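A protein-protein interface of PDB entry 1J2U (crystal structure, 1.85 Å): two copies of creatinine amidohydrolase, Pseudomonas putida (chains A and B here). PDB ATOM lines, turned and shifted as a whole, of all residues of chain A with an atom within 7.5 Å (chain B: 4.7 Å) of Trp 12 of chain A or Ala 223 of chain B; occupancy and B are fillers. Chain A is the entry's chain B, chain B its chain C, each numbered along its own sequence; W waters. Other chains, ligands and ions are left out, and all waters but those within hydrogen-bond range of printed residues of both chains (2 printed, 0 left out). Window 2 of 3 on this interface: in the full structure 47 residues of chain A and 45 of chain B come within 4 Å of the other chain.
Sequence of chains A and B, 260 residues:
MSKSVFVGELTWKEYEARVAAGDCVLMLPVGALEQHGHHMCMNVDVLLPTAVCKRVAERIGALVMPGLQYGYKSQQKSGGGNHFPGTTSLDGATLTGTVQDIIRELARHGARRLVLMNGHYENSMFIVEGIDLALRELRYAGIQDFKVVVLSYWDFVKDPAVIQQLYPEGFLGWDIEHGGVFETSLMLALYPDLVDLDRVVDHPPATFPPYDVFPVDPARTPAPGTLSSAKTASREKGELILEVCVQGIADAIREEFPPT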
ATOM      1  N   VAL A   7     -20.477  37.155  10.018  1.00  0.00           N
ATOM      2  CA  VAL A   7     -19.698  36.093  10.652  1.00  0.00           C
ATOM      3  C   VAL A   7     -20.595  34.934  11.096  1.00  0.00           C
ATOM      4  O   VAL A   7     -20.255  33.780  10.920  1.00  0.00           O
ATOM      5  CB  VAL A   7     -18.903  36.636  11.862  1.00  0.00           C
ATOM      6  CG1 VAL A   7     -18.258  35.519  12.638  1.00  0.00           C
ATOM      7  CG2 VAL A   7     -17.860  37.639  11.410  1.00  0.00           C
ATOM      8  N   LEU A  10     -21.203  32.396   8.402  1.00  0.00           N
ATOM      9  CA  LEU A  10     -20.045  31.687   7.862  1.00  0.00           C
ATOM     10  C   LEU A  10     -19.737  30.440   8.681  1.00  0.00           C
ATOM     11  O   LEU A  10     -20.148  30.346   9.824  1.00  0.00           O
ATOM     12  CB  LEU A  10     -18.820  32.584   7.901  1.00  0.00           C
ATOM     13  CG  LEU A  10     -18.838  33.885   7.092  1.00  0.00           C
ATOM     14  CD1 LEU A  10     -17.515  34.584   7.286  1.00  0.00           C
ATOM     15  CD2 LEU A  10     -19.096  33.616   5.627  1.00  0.00           C
ATOM     16  N   THR A  11     -19.009  29.488   8.096  1.00  0.00           N
ATOM     17  CA  THR A  11     -18.478  28.360   8.859  1.00  0.00           C
ATOM     18  C   THR A  11     -17.197  28.822   9.537  1.00  0.00           C
ATOM     19  O   THR A  11     -16.565  29.806   9.130  1.00  0.00           O
ATOM     20  CB  THR A  11     -18.099  27.160   7.946  1.00  0.00           C
ATOM     21  OG1 THR A  11     -17.013  27.545   7.098  1.00  0.00           O
ATOM     22  CG2 THR A  11     -19.231  26.767   6.990  1.00  0.00           C
ATOM     23  N   TRP A  12     -16.765  28.097  10.556  1.00  0.00           N
ATOM     24  CA  TRP A  12     -15.539  28.484  11.221  1.00  0.00           C
ATOM     25  C   TRP A  12     -14.345  28.434  10.284  1.00  0.00           C
ATOM     26  O   TRP A  12     -13.428  29.223  10.424  1.00  0.00           O
ATOM     27  CB  TRP A  12     -15.302  27.667  12.481  1.00  0.00           C
ATOM     28  CG  TRP A  12     -14.812  26.268  12.315  1.00  0.00           C
ATOM     29  CD1 TRP A  12     -15.567  25.138  12.324  1.00  0.00           C
ATOM     30  CD2 TRP A  12     -13.449  25.838  12.211  1.00  0.00           C
ATOM     31  NE1 TRP A  12     -14.764  24.029  12.216  1.00  0.00           N
ATOM     32  CE2 TRP A  12     -13.459  24.432  12.136  1.00  0.00           C
ATOM     33  CE3 TRP A  12     -12.218  26.500  12.142  1.00  0.00           C
ATOM     34  CZ2 TRP A  12     -12.288  23.680  12.014  1.00  0.00           C
ATOM     35  CZ3 TRP A  12     -11.067  25.757  12.021  1.00  0.00           C
ATOM     36  CH2 TRP A  12     -11.108  24.361  11.948  1.00  0.00           C
ATOM     37  N   LYS A  13     -14.366  27.523   9.318  1.00  0.00           N
ATOM     38  CA  LYS A  13     -13.274  27.435   8.339  1.00  0.00           C
ATOM     39  C   LYS A  13     -13.218  28.670   7.443  1.00  0.00           C
ATOM     40  O   LYS A  13     -12.137  29.173   7.136  1.00  0.00           O
ATOM     41  CB  LYS A  13     -13.440  26.191   7.469  1.00  0.00           C
ATOM     42  CG  LYS A  13     -13.301  24.903   8.244  1.00  0.00           C
ATOM     43  CD  LYS A  13     -11.887  24.681   8.651  1.00  0.00           C
ATOM     44  CE  LYS A  13     -11.020  24.305   7.456  1.00  0.00           C
ATOM     45  NZ  LYS A  13      -9.650  23.949   7.932  1.00  0.00           N
ATOM     46  N   GLU A  14     -14.385  29.140   7.026  1.00  0.00           N
ATOM     47  CA  GLU A  14     -14.498  30.321   6.174  1.00  0.00           C
ATOM     48  C   GLU A  14     -13.968  31.539   6.939  1.00  0.00           C
ATOM     49  O   GLU A  14     -13.162  32.313   6.432  1.00  0.00           O
ATOM     50  CB  GLU A  14     -15.949  30.520   5.733  1.00  0.00           C
ATOM     51  CG  GLU A  14     -16.403  29.519   4.660  1.00  0.00           C
ATOM     52  CD  GLU A  14     -17.915  29.422   4.447  1.00  0.00           C
ATOM     53  OE1 GLU A  14     -18.307  28.767   3.445  1.00  0.00           O
ATOM     54  OE2 GLU A  14     -18.729  29.949   5.245  1.00  0.00           O
ATOM     55  N   TYR A  15     -14.426  31.700   8.172  1.00  0.00           N
ATOM     56  CA  TYR A  15     -13.952  32.794   9.011  1.00  0.00           C
ATOM     57  C   TYR A  15     -12.434  32.719   9.235  1.00  0.00           C
ATOM     58  O   TYR A  15     -11.733  33.715   9.084  1.00  0.00           O
ATOM     59  CB  TYR A  15     -14.710  32.767  10.339  1.00  0.00           C
ATOM     60  CG  TYR A  15     -14.223  33.780  11.356  1.00  0.00           C
ATOM     61  CD1 TYR A  15     -14.675  35.092  11.340  1.00  0.00           C
ATOM     62  CD2 TYR A  15     -13.328  33.419  12.330  1.00  0.00           C
ATOM     63  CE1 TYR A  15     -14.228  36.006  12.265  1.00  0.00           C
ATOM     64  CE2 TYR A  15     -12.879  34.322  13.262  1.00  0.00           C
ATOM     65  CZ  TYR A  15     -13.335  35.610  13.225  1.00  0.00           C
ATOM     66  OH  TYR A  15     -12.877  36.474  14.169  1.00  0.00           O
ATOM     67  N   GLU A  16     -11.937  31.540   9.592  1.00  0.00           N
ATOM     68  CA  GLU A  16     -10.502  31.318   9.784  1.00  0.00           C
ATOM     69  C   GLU A  16      -9.707  31.780   8.566  1.00  0.00           C
ATOM     70  O   GLU A  16      -8.714  32.494   8.682  1.00  0.00           O
ATOM     71  CB  GLU A  16     -10.229  29.836  10.041  1.00  0.00           C
ATOM     72  CG  GLU A  16      -8.765  29.517  10.288  1.00  0.00           C
ATOM     73  CD  GLU A  16      -8.518  28.050  10.539  1.00  0.00           C
ATOM     74  OE1 GLU A  16      -7.867  27.729  11.547  1.00  0.00           O
ATOM     75  OE2 GLU A  16      -8.975  27.221   9.724  1.00  0.00           O
ATOM     76  N   ALA A  17     -10.166  31.397   7.387  1.00  0.00           N
ATOM     77  CA  ALA A  17      -9.474  31.761   6.149  1.00  0.00           C
ATOM     78  C   ALA A  17      -9.486  33.267   5.931  1.00  0.00           C
ATOM     79  O   ALA A  17      -8.496  33.858   5.476  1.00  0.00           O
ATOM     80  CB  ALA A  17     -10.108  31.042   4.958  1.00  0.00           C
ATOM     81  N   ARG A  18     -10.605  33.908   6.252  1.00  0.00           N
ATOM     82  CA  ARG A  18     -10.687  35.348   6.081  1.00  0.00           C
ATOM     83  C   ARG A  18      -9.724  36.067   7.021  1.00  0.00           C
ATOM     84  O   ARG A  18      -9.053  37.015   6.619  1.00  0.00           O
ATOM     85  CB  ARG A  18     -12.118  35.847   6.261  1.00  0.00           C
ATOM     86  CG  ARG A  18     -13.017  35.523   5.090  1.00  0.00           C
ATOM     87  CD  ARG A  18     -12.579  36.170   3.784  1.00  0.00           C
ATOM     88  NE  ARG A  18     -12.843  37.607   3.799  1.00  0.00           N
ATOM     89  CZ  ARG A  18     -14.030  38.149   3.572  1.00  0.00           C
ATOM     90  NH1 ARG A  18     -15.076  37.386   3.301  1.00  0.00           N
ATOM     91  NH2 ARG A  18     -14.173  39.465   3.606  1.00  0.00           N
ATOM     92  N   GLN B  35     -18.327  27.670  16.498  1.00  0.00           N
ATOM     93  CA  GLN B  35     -18.059  26.784  15.373  1.00  0.00           C
ATOM     94  C   GLN B  35     -19.057  25.627  15.386  1.00  0.00           C
ATOM     95  O   GLN B  35     -19.419  25.107  16.456  1.00  0.00           O
ATOM     96  CB  GLN B  35     -16.620  26.259  15.439  1.00  0.00           C
ATOM     97  CG  GLN B  35     -16.329  25.299  16.601  1.00  0.00           C
ATOM     98  CD  GLN B  35     -16.721  23.844  16.291  1.00  0.00           C
ATOM     99  OE1 GLN B  35     -16.863  23.462  15.116  1.00  0.00           O
ATOM    100  NE2 GLN B  35     -16.871  23.028  17.344  1.00  0.00           N
ATOM    101  N   HIS B  36     -19.563  25.276  14.208  1.00  0.00           N
ATOM    102  CA  HIS B  36     -20.445  24.119  14.073  1.00  0.00           C
ATOM    103  C   HIS B  36     -20.043  23.272  12.863  1.00  0.00           C
ATOM    104  O   HIS B  36     -20.879  22.935  12.038  1.00  0.00           O
ATOM    105  CB  HIS B  36     -21.914  24.500  13.943  1.00  0.00           C
ATOM    106  CG  HIS B  36     -22.611  24.728  15.246  1.00  0.00           C
ATOM    107  ND1 HIS B  36     -22.482  25.900  15.964  1.00  0.00           N
ATOM    108  CD2 HIS B  36     -23.491  23.961  15.929  1.00  0.00           C
ATOM    109  CE1 HIS B  36     -23.228  25.824  17.056  1.00  0.00           C
ATOM    110  NE2 HIS B  36     -23.862  24.660  17.052  1.00  0.00           N
ATOM    111  N   GLY B  37     -18.759  22.956  12.754  1.00  0.00           N
ATOM    112  CA  GLY B  37     -18.273  22.070  11.710  1.00  0.00           C
ATOM    113  C   GLY B  37     -17.993  22.760  10.400  1.00  0.00           C
ATOM    114  O   GLY B  37     -18.054  23.985  10.297  1.00  0.00           O
ATOM    115  N   HIS B  38     -17.677  21.945   9.394  1.00  0.00           N
ATOM    116  CA  HIS B  38     -17.351  22.427   8.056  1.00  0.00           C
ATOM    117  C   HIS B  38     -18.586  22.712   7.223  1.00  0.00           C
ATOM    118  O   HIS B  38     -18.524  23.449   6.257  1.00  0.00           O
ATOM    119  CB  HIS B  38     -16.537  21.365   7.312  1.00  0.00           C
ATOM    120  CG  HIS B  38     -15.153  21.166   7.840  1.00  0.00           C
ATOM    121  ND1 HIS B  38     -14.159  20.562   7.097  1.00  0.00           N
ATOM    122  CD2 HIS B  38     -14.592  21.479   9.033  1.00  0.00           C
ATOM    123  CE1 HIS B  38     -13.043  20.522   7.805  1.00  0.00           C
ATOM    124  NE2 HIS B  38     -13.278  21.069   8.985  1.00  0.00           N
ATOM    125  N   MET B  42     -22.038  29.518  12.149  1.00  0.00           N
ATOM    126  CA  MET B  42     -21.735  29.643  13.578  1.00  0.00           C
ATOM    127  C   MET B  42     -22.822  30.262  14.473  1.00  0.00           C
ATOM    128  O   MET B  42     -22.670  30.253  15.697  1.00  0.00           O
ATOM    129  CB  MET B  42     -20.422  30.422  13.748  1.00  0.00           C
ATOM    130  CG  MET B  42     -19.214  29.727  13.105  1.00  0.00           C
ATOM    131  SD  MET B  42     -17.666  30.487  13.479  1.00  0.00           S
ATOM    132  CE  MET B  42     -17.661  31.815  12.280  1.00  0.00           C
ATOM    133  N   PHE B  84     -11.216  26.945  19.210  1.00  0.00           N
ATOM    134  CA  PHE B  84     -11.535  27.136  17.797  1.00  0.00           C
ATOM    135  C   PHE B  84     -11.653  28.607  17.421  1.00  0.00           C
ATOM    136  O   PHE B  84     -12.088  29.438  18.234  1.00  0.00           O
ATOM    137  CB  PHE B  84     -12.851  26.456  17.420  1.00  0.00           C
ATOM    138  CG  PHE B  84     -12.722  24.973  17.167  1.00  0.00           C
ATOM    139  CD1 PHE B  84     -12.727  24.073  18.218  1.00  0.00           C
ATOM    140  CD2 PHE B  84     -12.620  24.483  15.873  1.00  0.00           C
ATOM    141  CE1 PHE B  84     -12.618  22.701  17.982  1.00  0.00           C
ATOM    142  CE2 PHE B  84     -12.492  23.111  15.636  1.00  0.00           C
ATOM    143  CZ  PHE B  84     -12.494  22.228  16.691  1.00  0.00           C
ATOM    144  N   PRO B  85     -11.300  28.917  16.175  1.00  0.00           N
ATOM    145  CA  PRO B  85     -11.535  30.250  15.620  1.00  0.00           C
ATOM    146  C   PRO B  85     -13.040  30.466  15.470  1.00  0.00           C
ATOM    147  O   PRO B  85     -13.756  29.475  15.404  1.00  0.00           O
ATOM    148  CB  PRO B  85     -10.931  30.168  14.217  1.00  0.00           C
ATOM    149  CG  PRO B  85     -10.152  28.890  14.162  1.00  0.00           C
ATOM    150  CD  PRO B  85     -10.696  27.998  15.199  1.00  0.00           C
ATOM    151  N   THR B 221     -10.712  16.624  20.246  1.00  0.00           N
ATOM    152  CA  THR B 221     -11.920  16.995  19.517  1.00  0.00           C
ATOM    153  C   THR B 221     -11.719  16.578  18.061  1.00  0.00           C
ATOM    154  O   THR B 221     -10.640  16.814  17.515  1.00  0.00           O
ATOM    155  CB  THR B 221     -12.146  18.543  19.543  1.00  0.00           C
ATOM    156  OG1 THR B 221     -12.369  18.997  20.879  1.00  0.00           O
ATOM    157  CG2 THR B 221     -13.428  18.924  18.806  1.00  0.00           C
ATOM    158  N   PRO B 222     -12.724  15.975  17.420  1.00  0.00           N
ATOM    159  CA  PRO B 222     -12.607  15.647  15.994  1.00  0.00           C
ATOM    160  C   PRO B 222     -12.270  16.908  15.215  1.00  0.00           C
ATOM    161  O   PRO B 222     -12.859  17.960  15.485  1.00  0.00           O
ATOM    162  CB  PRO B 222     -13.993  15.129  15.623  1.00  0.00           C
ATOM    163  CG  PRO B 222     -14.578  14.661  16.888  1.00  0.00           C
ATOM    164  CD  PRO B 222     -14.020  15.555  17.974  1.00  0.00           C
ATOM    165  N   ALA B 223     -11.331  16.794  14.278  1.00  0.00           N
ATOM    166  CA  ALA B 223     -10.803  17.937  13.521  1.00  0.00           C
ATOM    167  C   ALA B 223     -11.839  18.952  13.018  1.00  0.00           C
ATOM    168  O   ALA B 223     -11.610  20.143  13.124  1.00  0.00           O
ATOM    169  CB  ALA B 223      -9.939  17.440  12.348  1.00  0.00           C
ATOM    170  N   PRO B 224     -12.956  18.502  12.461  1.00  0.00           N
ATOM    171  CA  PRO B 224     -13.970  19.432  11.944  1.00  0.00           C
ATOM    172  C   PRO B 224     -14.690  20.222  13.024  1.00  0.00           C
ATOM    173  O   PRO B 224     -15.327  21.209  12.689  1.00  0.00           O
ATOM    174  CB  PRO B 224     -14.976  18.520  11.240  1.00  0.00           C
ATOM    175  CG  PRO B 224     -14.343  17.171  11.170  1.00  0.00           C
ATOM    176  CD  PRO B 224     -13.343  17.095  12.260  1.00  0.00           C
ATOM    177  N   GLY B 225     -14.627  19.774  14.274  1.00  0.00           N
ATOM    178  CA  GLY B 225     -15.285  20.467  15.374  1.00  0.00           C
ATOM    179  C   GLY B 225     -16.618  19.883  15.805  1.00  0.00           C
ATOM    180  O   GLY B 225     -17.137  20.215  16.869  1.00  0.00           O
HETATM  181  O   HOH W   1     -18.919  26.191  11.591  1.00  0.00           O
HETATM  182  O   HOH W   2     -16.534  25.214   5.561  1.00  0.00           O
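Of the 10 printed residues of chain A, 7 touch a printed residue of chain B.
Printed residues of chain A that touch a printed residue of chain B: Val 7, Leu 10, Thr 11, Trp 12, Lys 13, Tyr 15 and Glu 16.
Hydrophobic or aromatic side chains of chain A that line the printed part of chain B: Val 7, Trp 12 and Tyr 15.
Of the 12 printed residues of chain B, 8 touch a printed residue of chain A.
Printed residues of chain B that touch a printed residue of chain A: Gln 35, Gly 37, His 38, Met 42, Phe 84, Pro 85, Ala 223 and Pro 224.
Among the printed residues, 15 pairs touch across the chains.
No position is printed for both chains.
Water W1 lies within hydrogen-bond range of the backbone carbonyl oxygen (O) of Gly 37 of chain B (2.7 Å), the backbone NH (N) of His 36 of chain B (2.8 Å) and the backbone NH (N) of Trp 12 of chain A (3.1 Å).
Water W2 lies within hydrogen-bond range of the backbone carbonyl oxygen of His 38 of chain B and the side-chain hydroxyl of Thr 11 of chain A.
The backbone carbonyl oxygen of Leu 10 of chain A lies within hydrogen-bond range of the backbone NH of Met 42 of chain B (3.1 Å).
The backbone carbonyl oxygen (O) of Pro 224 of chain B is in hydrogen-bond range of the indole nitrogen (NE1) of Trp 12 of chain A, 2.9 Å away.
Of chain B, only Gln 35 (3.5 Å), Gly 37 (3.4 Å), Met 42 (3.7 Å), Phe 84 (3.7 Å), Pro 85 (3.7 Å), Ala 223 (3.8 Å) and Pro 224 (2.9 Å) come within 4 Å of Trp 12 of chain A.
Of the printed residues of chain B, Lys 13 of chain A touches His 38 (3.7 Å).
Glu 14 of chain A touches none of the printed residues of chain B.
Of the printed residues of chain A, Gln 35 of chain B touches Trp 12.
Of the printed residues of chain A, His 38 of chain B touches Thr 11 and Lys 13.
Of the printed residues of chain A, Met 42 of chain B touches Val 7 (3.5 Å), Leu 10 (3.1 Å), Thr 11 (3.9 Å), Trp 12 (3.7 Å) and Tyr 15 (3.7 Å).
Of the printed residues of chain A, Ala 223 of chain B touches Trp 12.
Gly 225 of chain B touches none of the printed residues of chain A.
The nearest residue of chain B that does not touch Trp 12 of chain A is His 38 of chain B (4.1 Å).
The nearest residue of chain A that does not touch Ala 223 of chain B is Lys 13 of chain A (6.4 Å).
The side-chain hydroxyl of Thr 11 of chain A sits close to the backbone NH of Lys 13 of chain A (3.5 Å).
OE2 of Glu 14 of chain A is in hydrogen-bond range of N of Thr 11 of chain A.
NZ of Lys 13 of chain A lies within salt-bridge range of OE2 of Glu 16 of chain A, at 3.8 Å.
OE1 of Gln 35 of chain B sits at hydrogen-bond distance from N of Gly 37 of chain B, at 3.1 Å.
NE2 of Gln 35 of chain B lies within hydrogen-bond range of O of Gly 225 of chain B (2.9 Å).
Among the printed residues, merely in contact across the chains: Val 7 of chain A with Met 42 of chain B, Thr 11 of chain A with Gly 37 of chain B, Thr 11 of chain A with His 38 of chain B, Thr 11 of chain A with Met 42 of chain B, Trp 12 of chain A with Gln 35 of chain B, Trp 12 of chain A with Gly 37 of chain B, Trp 12 of chain A with Met 42 of chain B, Trp 12 of chain A with Phe 84 of chain B, Trp 12 of chain A with Pro 85 of chain B, Trp 12 of chain A with Ala 223 of chain B, Lys 13 of chain A with His 38 of chain B, Tyr 15 of chain A with Met 42 of chain B and Glu 16 of chain A with Pro 85 of chain B.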
